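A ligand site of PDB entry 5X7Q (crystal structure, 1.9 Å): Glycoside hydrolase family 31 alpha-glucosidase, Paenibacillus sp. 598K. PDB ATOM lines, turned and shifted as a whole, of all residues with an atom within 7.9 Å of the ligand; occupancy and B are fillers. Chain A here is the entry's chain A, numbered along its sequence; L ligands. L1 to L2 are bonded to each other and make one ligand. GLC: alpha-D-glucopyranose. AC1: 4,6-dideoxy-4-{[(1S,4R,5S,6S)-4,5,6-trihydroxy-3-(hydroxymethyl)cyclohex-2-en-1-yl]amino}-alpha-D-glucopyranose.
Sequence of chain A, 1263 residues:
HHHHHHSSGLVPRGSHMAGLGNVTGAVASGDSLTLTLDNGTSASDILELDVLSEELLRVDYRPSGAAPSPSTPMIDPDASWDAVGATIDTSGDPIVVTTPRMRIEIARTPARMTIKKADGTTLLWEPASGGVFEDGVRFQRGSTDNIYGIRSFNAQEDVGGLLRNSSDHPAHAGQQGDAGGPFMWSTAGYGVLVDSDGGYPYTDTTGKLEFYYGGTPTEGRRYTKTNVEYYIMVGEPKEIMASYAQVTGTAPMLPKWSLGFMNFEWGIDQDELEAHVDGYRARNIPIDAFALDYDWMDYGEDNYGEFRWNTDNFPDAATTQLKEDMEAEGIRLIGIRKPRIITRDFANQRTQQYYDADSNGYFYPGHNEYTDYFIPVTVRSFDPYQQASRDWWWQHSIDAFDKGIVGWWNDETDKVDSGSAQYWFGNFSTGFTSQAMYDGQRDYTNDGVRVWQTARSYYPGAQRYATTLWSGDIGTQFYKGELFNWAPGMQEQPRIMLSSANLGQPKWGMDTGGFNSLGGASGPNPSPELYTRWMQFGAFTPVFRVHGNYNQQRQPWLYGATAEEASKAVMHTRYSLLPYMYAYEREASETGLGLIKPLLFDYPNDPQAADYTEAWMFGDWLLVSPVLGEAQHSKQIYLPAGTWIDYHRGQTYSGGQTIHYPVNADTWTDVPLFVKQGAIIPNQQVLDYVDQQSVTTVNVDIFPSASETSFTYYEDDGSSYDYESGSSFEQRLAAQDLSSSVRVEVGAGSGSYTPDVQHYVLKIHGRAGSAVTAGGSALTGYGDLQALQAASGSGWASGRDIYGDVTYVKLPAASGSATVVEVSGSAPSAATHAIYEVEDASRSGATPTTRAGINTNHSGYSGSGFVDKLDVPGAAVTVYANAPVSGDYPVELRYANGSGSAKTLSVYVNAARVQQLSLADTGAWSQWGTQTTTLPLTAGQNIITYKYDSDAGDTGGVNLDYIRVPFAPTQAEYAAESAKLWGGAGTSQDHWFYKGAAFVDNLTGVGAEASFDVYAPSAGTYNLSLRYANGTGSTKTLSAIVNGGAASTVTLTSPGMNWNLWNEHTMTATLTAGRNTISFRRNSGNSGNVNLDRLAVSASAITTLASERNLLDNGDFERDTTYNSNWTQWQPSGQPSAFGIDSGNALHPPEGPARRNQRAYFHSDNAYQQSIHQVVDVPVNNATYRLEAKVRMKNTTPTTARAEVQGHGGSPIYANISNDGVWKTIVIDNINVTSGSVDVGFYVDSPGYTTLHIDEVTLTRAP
The side-chain carboxylate (OE2) of Glu 1204 lies within hydrogen-bond range of an oxygen (O4) of AC1 L2 (2.6 Å).
OG of Ser 1171 sits at hydrogen-bond distance from O2B of AC1 L2, at 2.7 Å.
NE2 of His 1173 lies within hydrogen-bond range of O3B of AC1 L2, 2.9 Å away.
An oxygen (O4) of AC1 L2 is in hydrogen-bond range of the guanidinium group (NH2) of Arg 1202 (3.1 Å).
The side-chain carboxylate of Glu 1204 lies within salt-bridge range of the guanidinium group of Arg 1202 (2.7 Å).
OE1 of Gln 1206 lies close to OE1 of Glu 1204 (3.2 Å).
The backbone NH (N) of Glu 1204 sits at hydrogen-bond distance from the backbone carbonyl oxygen (O) of Gly 1241, at 2.8 Å.
A ring nitrogen (ND1) of His 1173 is in hydrogen-bond range of the side-chain carboxylate (OD1) of Asp 1239 (2.8 Å).
The backbone carbonyl oxygen (O) of His 1173 lies within hydrogen-bond range of the backbone NH (N) of Thr 1128 (2.7 Å).
The backbone carbonyl oxygen (O) of Arg 1202 sits at hydrogen-bond distance from the backbone NH (N) of Tyr 1243 (2.9 Å).
The side-chain hydroxyl (OH) of Tyr 1243 sits at hydrogen-bond distance from the side-chain amide oxygen (OE1) of Gln 1169.
O of Trp 1130 lies within hydrogen-bond range of NE2 of Gln 1170, 3.0 Å away.
Merely in contact with the ligand: Tyr 1243 and Trp 1130.
Along chain A the residues within 4 Å of the ligand span positions 1130 to 1243.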
ATOM      1  N   THR A1128       6.093   2.303 -22.458  1.00  0.00           N
ATOM      2  CA  THR A1128       7.074   3.389 -22.377  1.00  0.00           C
ATOM      3  C   THR A1128       8.006   3.118 -21.213  1.00  0.00           C
ATOM      4  O   THR A1128       7.696   2.298 -20.335  1.00  0.00           O
ATOM      5  CB  THR A1128       6.395   4.755 -22.158  1.00  0.00           C
ATOM      6  OG1 THR A1128       5.661   4.746 -20.919  1.00  0.00           O
ATOM      7  CG2 THR A1128       5.428   5.055 -23.283  1.00  0.00           C
ATOM      8  N   GLN A1129       9.149   3.796 -21.208  1.00  0.00           N
ATOM      9  CA  GLN A1129      10.158   3.621 -20.158  1.00  0.00           C
ATOM     10  C   GLN A1129      10.599   4.946 -19.559  1.00  0.00           C
ATOM     11  O   GLN A1129      10.482   5.986 -20.195  1.00  0.00           O
ATOM     12  CB  GLN A1129      11.374   2.851 -20.687  1.00  0.00           C
ATOM     13  CG  GLN A1129      12.158   3.541 -21.786  1.00  0.00           C
ATOM     14  CD  GLN A1129      13.430   2.804 -22.112  1.00  0.00           C
ATOM     15  OE1 GLN A1129      14.328   2.694 -21.274  1.00  0.00           O
ATOM     16  NE2 GLN A1129      13.517   2.272 -23.323  1.00  0.00           N
ATOM     17  N   TRP A1130      11.087   4.878 -18.337  1.00  0.00           N
ATOM     18  CA  TRP A1130      11.683   6.039 -17.688  1.00  0.00           C
ATOM     19  C   TRP A1130      12.902   5.611 -16.880  1.00  0.00           C
ATOM     20  O   TRP A1130      12.935   4.515 -16.289  1.00  0.00           O
ATOM     21  CB  TRP A1130      10.659   6.751 -16.788  1.00  0.00           C
ATOM     22  CG  TRP A1130      11.280   7.755 -15.871  1.00  0.00           C
ATOM     23  CD1 TRP A1130      11.433   9.094 -16.110  1.00  0.00           C
ATOM     24  CD2 TRP A1130      11.856   7.502 -14.582  1.00  0.00           C
ATOM     25  NE1 TRP A1130      12.063   9.697 -15.038  1.00  0.00           N
ATOM     26  CE2 TRP A1130      12.338   8.751 -14.092  1.00  0.00           C
ATOM     27  CE3 TRP A1130      12.019   6.355 -13.793  1.00  0.00           C
ATOM     28  CZ2 TRP A1130      12.961   8.868 -12.837  1.00  0.00           C
ATOM     29  CZ3 TRP A1130      12.642   6.470 -12.553  1.00  0.00           C
ATOM     30  CH2 TRP A1130      13.103   7.720 -12.085  1.00  0.00           C
ATOM     31  N   GLN A1131      13.893   6.489 -16.888  1.00  0.00           N
ATOM     32  CA  GLN A1131      15.017   6.425 -15.968  1.00  0.00           C
ATOM     33  C   GLN A1131      15.408   7.872 -15.610  1.00  0.00           C
ATOM     34  O   GLN A1131      15.015   8.801 -16.320  1.00  0.00           O
ATOM     35  CB  GLN A1131      16.186   5.627 -16.586  1.00  0.00           C
ATOM     36  CG  GLN A1131      16.716   6.118 -17.924  1.00  0.00           C
ATOM     37  CD  GLN A1131      15.872   5.730 -19.127  1.00  0.00           C
ATOM     38  OE1 GLN A1131      15.722   6.517 -20.053  1.00  0.00           O
ATOM     39  NE2 GLN A1131      15.324   4.520 -19.124  1.00  0.00           N
ATOM     40  N   PRO A1132      16.151   8.063 -14.501  1.00  0.00           N
ATOM     41  CA  PRO A1132      16.606   9.424 -14.150  1.00  0.00           C
ATOM     42  C   PRO A1132      17.449  10.055 -15.260  1.00  0.00           C
ATOM     43  O   PRO A1132      18.240   9.354 -15.916  1.00  0.00           O
ATOM     44  CB  PRO A1132      17.480   9.208 -12.903  1.00  0.00           C
ATOM     45  CG  PRO A1132      17.071   7.888 -12.351  1.00  0.00           C
ATOM     46  CD  PRO A1132      16.646   7.059 -13.534  1.00  0.00           C
ATOM     47  N   GLN A1169      17.794   3.472 -11.211  1.00  0.00           N
ATOM     48  CA  GLN A1169      16.348   3.475 -11.148  1.00  0.00           C
ATOM     49  C   GLN A1169      15.830   3.261 -12.571  1.00  0.00           C
ATOM     50  O   GLN A1169      16.424   3.740 -13.542  1.00  0.00           O
ATOM     51  CB  GLN A1169      15.806   4.807 -10.635  1.00  0.00           C
ATOM     52  CG  GLN A1169      16.149   5.109  -9.179  1.00  0.00           C
ATOM     53  CD  GLN A1169      15.541   6.413  -8.727  1.00  0.00           C
ATOM     54  OE1 GLN A1169      14.322   6.518  -8.554  1.00  0.00           O
ATOM     55  NE2 GLN A1169      16.371   7.425  -8.558  1.00  0.00           N
ATOM     56  N   GLN A1170      14.712   2.555 -12.686  1.00  0.00           N
ATOM     57  CA  GLN A1170      14.150   2.236 -13.994  1.00  0.00           C
ATOM     58  C   GLN A1170      12.690   1.862 -13.831  1.00  0.00           C
ATOM     59  O   GLN A1170      12.306   1.198 -12.856  1.00  0.00           O
ATOM     60  CB  GLN A1170      14.911   1.055 -14.633  1.00  0.00           C
ATOM     61  CG  GLN A1170      14.408   0.611 -16.014  1.00  0.00           C
ATOM     62  CD  GLN A1170      14.732   1.610 -17.098  1.00  0.00           C
ATOM     63  OE1 GLN A1170      15.889   1.987 -17.276  1.00  0.00           O
ATOM     64  NE2 GLN A1170      13.726   2.037 -17.844  1.00  0.00           N
ATOM     65  N   SER A1171      11.877   2.283 -14.800  1.00  0.00           N
ATOM     66  CA  SER A1171      10.498   1.831 -14.888  1.00  0.00           C
ATOM     67  C   SER A1171      10.094   1.603 -16.321  1.00  0.00           C
ATOM     68  O   SER A1171      10.696   2.164 -17.232  1.00  0.00           O
ATOM     69  CB  SER A1171       9.539   2.844 -14.248  1.00  0.00           C
ATOM     70  OG  SER A1171       9.454   4.015 -15.053  1.00  0.00           O
ATOM     71  N   ILE A1172       9.062   0.791 -16.496  1.00  0.00           N
ATOM     72  CA  ILE A1172       8.270   0.793 -17.708  1.00  0.00           C
ATOM     73  C   ILE A1172       6.825   0.999 -17.326  1.00  0.00           C
ATOM     74  O   ILE A1172       6.417   0.634 -16.219  1.00  0.00           O
ATOM     75  CB  ILE A1172       8.441  -0.500 -18.549  1.00  0.00           C
ATOM     76  CG1 ILE A1172       8.022  -1.742 -17.766  1.00  0.00           C
ATOM     77  CG2 ILE A1172       9.870  -0.597 -19.049  1.00  0.00           C
ATOM     78  CD1 ILE A1172       7.976  -3.003 -18.610  1.00  0.00           C
ATOM     79  N   HIS A1173       6.068   1.588 -18.241  1.00  0.00           N
ATOM     80  CA  HIS A1173       4.667   1.900 -18.010  1.00  0.00           C
ATOM     81  C   HIS A1173       3.886   1.690 -19.290  1.00  0.00           C
ATOM     82  O   HIS A1173       4.424   1.868 -20.372  1.00  0.00           O
ATOM     83  CB  HIS A1173       4.489   3.369 -17.561  1.00  0.00           C
ATOM     84  CG  HIS A1173       4.932   3.607 -16.150  1.00  0.00           C
ATOM     85  ND1 HIS A1173       4.184   3.218 -15.061  1.00  0.00           N
ATOM     86  CD2 HIS A1173       6.077   4.138 -15.657  1.00  0.00           C
ATOM     87  CE1 HIS A1173       4.830   3.510 -13.955  1.00  0.00           C
ATOM     88  NE2 HIS A1173       5.989   4.073 -14.282  1.00  0.00           N
ATOM     89  N   THR A1200      13.715  -0.650  -3.732  1.00  0.00           N
ATOM     90  CA  THR A1200      12.326  -0.770  -4.186  1.00  0.00           C
ATOM     91  C   THR A1200      12.269  -1.628  -5.444  1.00  0.00           C
ATOM     92  O   THR A1200      13.117  -1.496  -6.334  1.00  0.00           O
ATOM     93  CB  THR A1200      11.753   0.628  -4.500  1.00  0.00           C
ATOM     94  OG1 THR A1200      11.887   1.440  -3.334  1.00  0.00           O
ATOM     95  CG2 THR A1200      10.296   0.558  -4.898  1.00  0.00           C
ATOM     96  N   ARG A1202       8.674  -3.108  -7.566  1.00  0.00           N
ATOM     97  CA  ARG A1202       7.220  -3.255  -7.487  1.00  0.00           C
ATOM     98  C   ARG A1202       6.497  -3.109  -8.813  1.00  0.00           C
ATOM     99  O   ARG A1202       6.977  -2.411  -9.712  1.00  0.00           O
ATOM    100  CB  ARG A1202       6.672  -2.214  -6.514  1.00  0.00           C
ATOM    101  CG  ARG A1202       6.933  -0.783  -6.958  1.00  0.00           C
ATOM    102  CD  ARG A1202       6.586   0.198  -5.865  1.00  0.00           C
ATOM    103  NE  ARG A1202       6.783   1.580  -6.324  1.00  0.00           N
ATOM    104  CZ  ARG A1202       6.817   2.657  -5.538  1.00  0.00           C
ATOM    105  NH1 ARG A1202       6.646   2.535  -4.220  1.00  0.00           N
ATOM    106  NH2 ARG A1202       7.011   3.856  -6.055  1.00  0.00           N
ATOM    107  N   ALA A1203       5.342  -3.771  -8.892  1.00  0.00           N
ATOM    108  CA  ALA A1203       4.298  -3.430  -9.868  1.00  0.00           C
ATOM    109  C   ALA A1203       3.503  -2.228  -9.333  1.00  0.00           C
ATOM    110  O   ALA A1203       3.380  -2.061  -8.109  1.00  0.00           O
ATOM    111  CB  ALA A1203       3.382  -4.609 -10.099  1.00  0.00           C
ATOM    112  N   GLU A1204       2.994  -1.407 -10.257  1.00  0.00           N
ATOM    113  CA  GLU A1204       2.246  -0.180  -9.932  1.00  0.00           C
ATOM    114  C   GLU A1204       1.008  -0.028 -10.826  1.00  0.00           C
ATOM    115  O   GLU A1204       1.107  -0.171 -12.054  1.00  0.00           O
ATOM    116  CB  GLU A1204       3.123   1.050 -10.168  1.00  0.00           C
ATOM    117  CG  GLU A1204       4.481   0.970  -9.484  1.00  0.00           C
ATOM    118  CD  GLU A1204       5.294   2.229  -9.618  1.00  0.00           C
ATOM    119  OE1 GLU A1204       5.049   3.044 -10.550  1.00  0.00           O
ATOM    120  OE2 GLU A1204       6.222   2.390  -8.786  1.00  0.00           O
ATOM    121  N   GLN A1206      -1.954   2.940 -11.403  1.00  0.00           N
ATOM    122  CA  GLN A1206      -2.293   4.329 -11.080  1.00  0.00           C
ATOM    123  C   GLN A1206      -3.050   4.980 -12.248  1.00  0.00           C
ATOM    124  O   GLN A1206      -3.194   4.373 -13.302  1.00  0.00           O
ATOM    125  CB  GLN A1206      -1.034   5.118 -10.710  1.00  0.00           C
ATOM    126  CG  GLN A1206       0.046   5.177 -11.778  1.00  0.00           C
ATOM    127  CD  GLN A1206       1.425   5.368 -11.185  1.00  0.00           C
ATOM    128  OE1 GLN A1206       2.300   4.517 -11.314  1.00  0.00           O
ATOM    129  NE2 GLN A1206       1.622   6.494 -10.517  1.00  0.00           N
ATOM    130  N   PRO A1212      -2.500   5.524  -6.231  1.00  0.00           N
ATOM    131  CA  PRO A1212      -1.657   4.407  -6.685  1.00  0.00           C
ATOM    132  C   PRO A1212      -1.779   3.139  -5.841  1.00  0.00           C
ATOM    133  O   PRO A1212      -1.951   3.226  -4.620  1.00  0.00           O
ATOM    134  CB  PRO A1212      -0.247   4.987  -6.595  1.00  0.00           C
ATOM    135  CG  PRO A1212      -0.444   6.436  -6.901  1.00  0.00           C
ATOM    136  CD  PRO A1212      -1.761   6.805  -6.291  1.00  0.00           C
ATOM    137  N   TYR A1214       0.263  -0.508  -5.071  1.00  0.00           N
ATOM    138  CA  TYR A1214       1.579  -1.128  -5.206  1.00  0.00           C
ATOM    139  C   TYR A1214       1.556  -2.593  -4.837  1.00  0.00           C
ATOM    140  O   TYR A1214       0.804  -3.030  -3.955  1.00  0.00           O
ATOM    141  CB  TYR A1214       2.603  -0.392  -4.353  1.00  0.00           C
ATOM    142  CG  TYR A1214       2.789   1.069  -4.718  1.00  0.00           C
ATOM    143  CD1 TYR A1214       2.982   1.447  -6.039  1.00  0.00           C
ATOM    144  CD2 TYR A1214       2.794   2.063  -3.741  1.00  0.00           C
ATOM    145  CE1 TYR A1214       3.147   2.778  -6.384  1.00  0.00           C
ATOM    146  CE2 TYR A1214       2.959   3.396  -4.072  1.00  0.00           C
ATOM    147  CZ  TYR A1214       3.136   3.743  -5.388  1.00  0.00           C
ATOM    148  OH  TYR A1214       3.314   5.052  -5.751  1.00  0.00           O
ATOM    149  N   ASP A1239      -2.929   3.100 -15.899  1.00  0.00           N
ATOM    150  CA  ASP A1239      -1.492   3.022 -16.100  1.00  0.00           C
ATOM    151  C   ASP A1239      -1.008   1.827 -15.283  1.00  0.00           C
ATOM    152  O   ASP A1239      -1.164   1.807 -14.067  1.00  0.00           O
ATOM    153  CB  ASP A1239      -0.835   4.318 -15.621  1.00  0.00           C
ATOM    154  CG  ASP A1239       0.688   4.341 -15.772  1.00  0.00           C
ATOM    155  OD1 ASP A1239       1.388   3.311 -15.577  1.00  0.00           O
ATOM    156  OD2 ASP A1239       1.202   5.427 -16.072  1.00  0.00           O
ATOM    157  N   GLY A1241       2.477  -0.579 -14.482  1.00  0.00           N
ATOM    158  CA  GLY A1241       3.901  -0.367 -14.535  1.00  0.00           C
ATOM    159  C   GLY A1241       4.717  -1.210 -13.587  1.00  0.00           C
ATOM    160  O   GLY A1241       4.177  -1.921 -12.715  1.00  0.00           O
ATOM    161  N   PHE A1242       6.018  -1.126 -13.780  1.00  0.00           N
ATOM    162  CA  PHE A1242       7.005  -1.836 -12.978  1.00  0.00           C
ATOM    163  C   PHE A1242       8.167  -0.878 -12.736  1.00  0.00           C
ATOM    164  O   PHE A1242       8.613  -0.223 -13.687  1.00  0.00           O
ATOM    165  CB  PHE A1242       7.465  -3.099 -13.718  1.00  0.00           C
ATOM    166  CG  PHE A1242       6.360  -4.100 -13.923  1.00  0.00           C
ATOM    167  CD1 PHE A1242       6.056  -5.024 -12.935  1.00  0.00           C
ATOM    168  CD2 PHE A1242       5.587  -4.086 -15.079  1.00  0.00           C
ATOM    169  CE1 PHE A1242       5.008  -5.929 -13.089  1.00  0.00           C
ATOM    170  CE2 PHE A1242       4.549  -4.991 -15.247  1.00  0.00           C
ATOM    171  CZ  PHE A1242       4.264  -5.913 -14.259  1.00  0.00           C
ATOM    172  N   TYR A1243       8.636  -0.815 -11.491  1.00  0.00           N
ATOM    173  CA  TYR A1243       9.677   0.139 -11.065  1.00  0.00           C
ATOM    174  C   TYR A1243      10.690  -0.536 -10.153  1.00  0.00           C
ATOM    175  O   TYR A1243      10.315  -1.329  -9.273  1.00  0.00           O
ATOM    176  CB  TYR A1243       9.038   1.320 -10.352  1.00  0.00           C
ATOM    177  CG  TYR A1243       9.985   2.232  -9.600  1.00  0.00           C
ATOM    178  CD1 TYR A1243      10.918   3.015 -10.288  1.00  0.00           C
ATOM    179  CD2 TYR A1243       9.941   2.342  -8.215  1.00  0.00           C
ATOM    180  CE1 TYR A1243      11.783   3.867  -9.607  1.00  0.00           C
ATOM    181  CE2 TYR A1243      10.806   3.195  -7.520  1.00  0.00           C
ATOM    182  CZ  TYR A1243      11.713   3.953  -8.212  1.00  0.00           C
ATOM    183  OH  TYR A1243      12.579   4.797  -7.537  1.00  0.00           O
ATOM    184  N   VAL A1244      11.972  -0.250 -10.385  1.00  0.00           N
ATOM    185  CA  VAL A1244      13.057  -0.735  -9.530  1.00  0.00           C
ATOM    186  C   VAL A1244      13.966   0.430  -9.111  1.00  0.00           C
ATOM    187  O   VAL A1244      14.351   1.223  -9.955  1.00  0.00           O
ATOM    188  CB  VAL A1244      13.896  -1.831 -10.216  1.00  0.00           C
ATOM    189  CG1 VAL A1244      15.126  -2.198  -9.390  1.00  0.00           C
ATOM    190  CG2 VAL A1244      13.051  -3.083 -10.420  1.00  0.00           C
ATOM    191  N   ASP A1245      14.293   0.495  -7.811  1.00  0.00           N
ATOM    192  CA  ASP A1245      15.369   1.356  -7.271  1.00  0.00           C
ATOM    193  C   ASP A1245      16.445   0.452  -6.680  1.00  0.00           C
ATOM    194  O   ASP A1245      16.234  -0.152  -5.632  1.00  0.00           O
ATOM    195  CB  ASP A1245      14.796   2.293  -6.196  1.00  0.00           C
ATOM    196  CG  ASP A1245      15.856   3.198  -5.548  1.00  0.00           C
ATOM    197  OD1 ASP A1245      17.038   3.199  -5.975  1.00  0.00           O
ATOM    198  OD2 ASP A1245      15.489   3.909  -4.585  1.00  0.00           O
HETATM  199  O4  GLC L   1       6.680  12.169 -14.579  1.00  0.00           O
HETATM  200  C1  AC1 L   2       7.918  11.530 -14.941  1.00  0.00           C
HETATM  201  O2  AC1 L   2       6.678  10.058 -16.450  1.00  0.00           O
HETATM  202  C2  AC1 L   2       7.685  10.100 -15.441  1.00  0.00           C
HETATM  203  C4A AC1 L   2       8.100   5.305  -9.798  1.00  0.00           C
HETATM  204  C3  AC1 L   2       7.291   9.166 -14.289  1.00  0.00           C
HETATM  205  O3  AC1 L   2       7.125   7.834 -14.774  1.00  0.00           O
HETATM  206  C4  AC1 L   2       8.376   9.228 -13.224  1.00  0.00           C
HETATM  207  N4A AC1 L   2       8.099   8.323 -12.139  1.00  0.00           N
HETATM  208  C5  AC1 L   2       8.505  10.673 -12.715  1.00  0.00           C
HETATM  209  O5  AC1 L   2       8.816  11.553 -13.810  1.00  0.00           O
HETATM  210  C6  AC1 L   2       9.611  10.801 -11.667  1.00  0.00           C
HETATM  211  C1B AC1 L   2       9.090   7.385 -11.637  1.00  0.00           C
HETATM  212  C2B AC1 L   2       8.745   5.961 -12.083  1.00  0.00           C
HETATM  213  O2B AC1 L   2       8.373   5.926 -13.466  1.00  0.00           O
HETATM  214  C3B AC1 L   2       7.615   5.418 -11.236  1.00  0.00           C
HETATM  215  O3B AC1 L   2       7.230   4.129 -11.703  1.00  0.00           O
HETATM  216  O4  AC1 L   2       7.039   4.843  -8.962  1.00  0.00           O
HETATM  217  C5B AC1 L   2       8.678   6.587  -9.283  1.00  0.00           C
HETATM  218  C7B AC1 L   2       9.175   7.512 -10.131  1.00  0.00           C
HETATM  219  C6B AC1 L   2       8.694   6.776  -7.773  1.00  0.00           C
HETATM  220  O6B AC1 L   2       9.455   7.918  -7.354  1.00  0.00           O
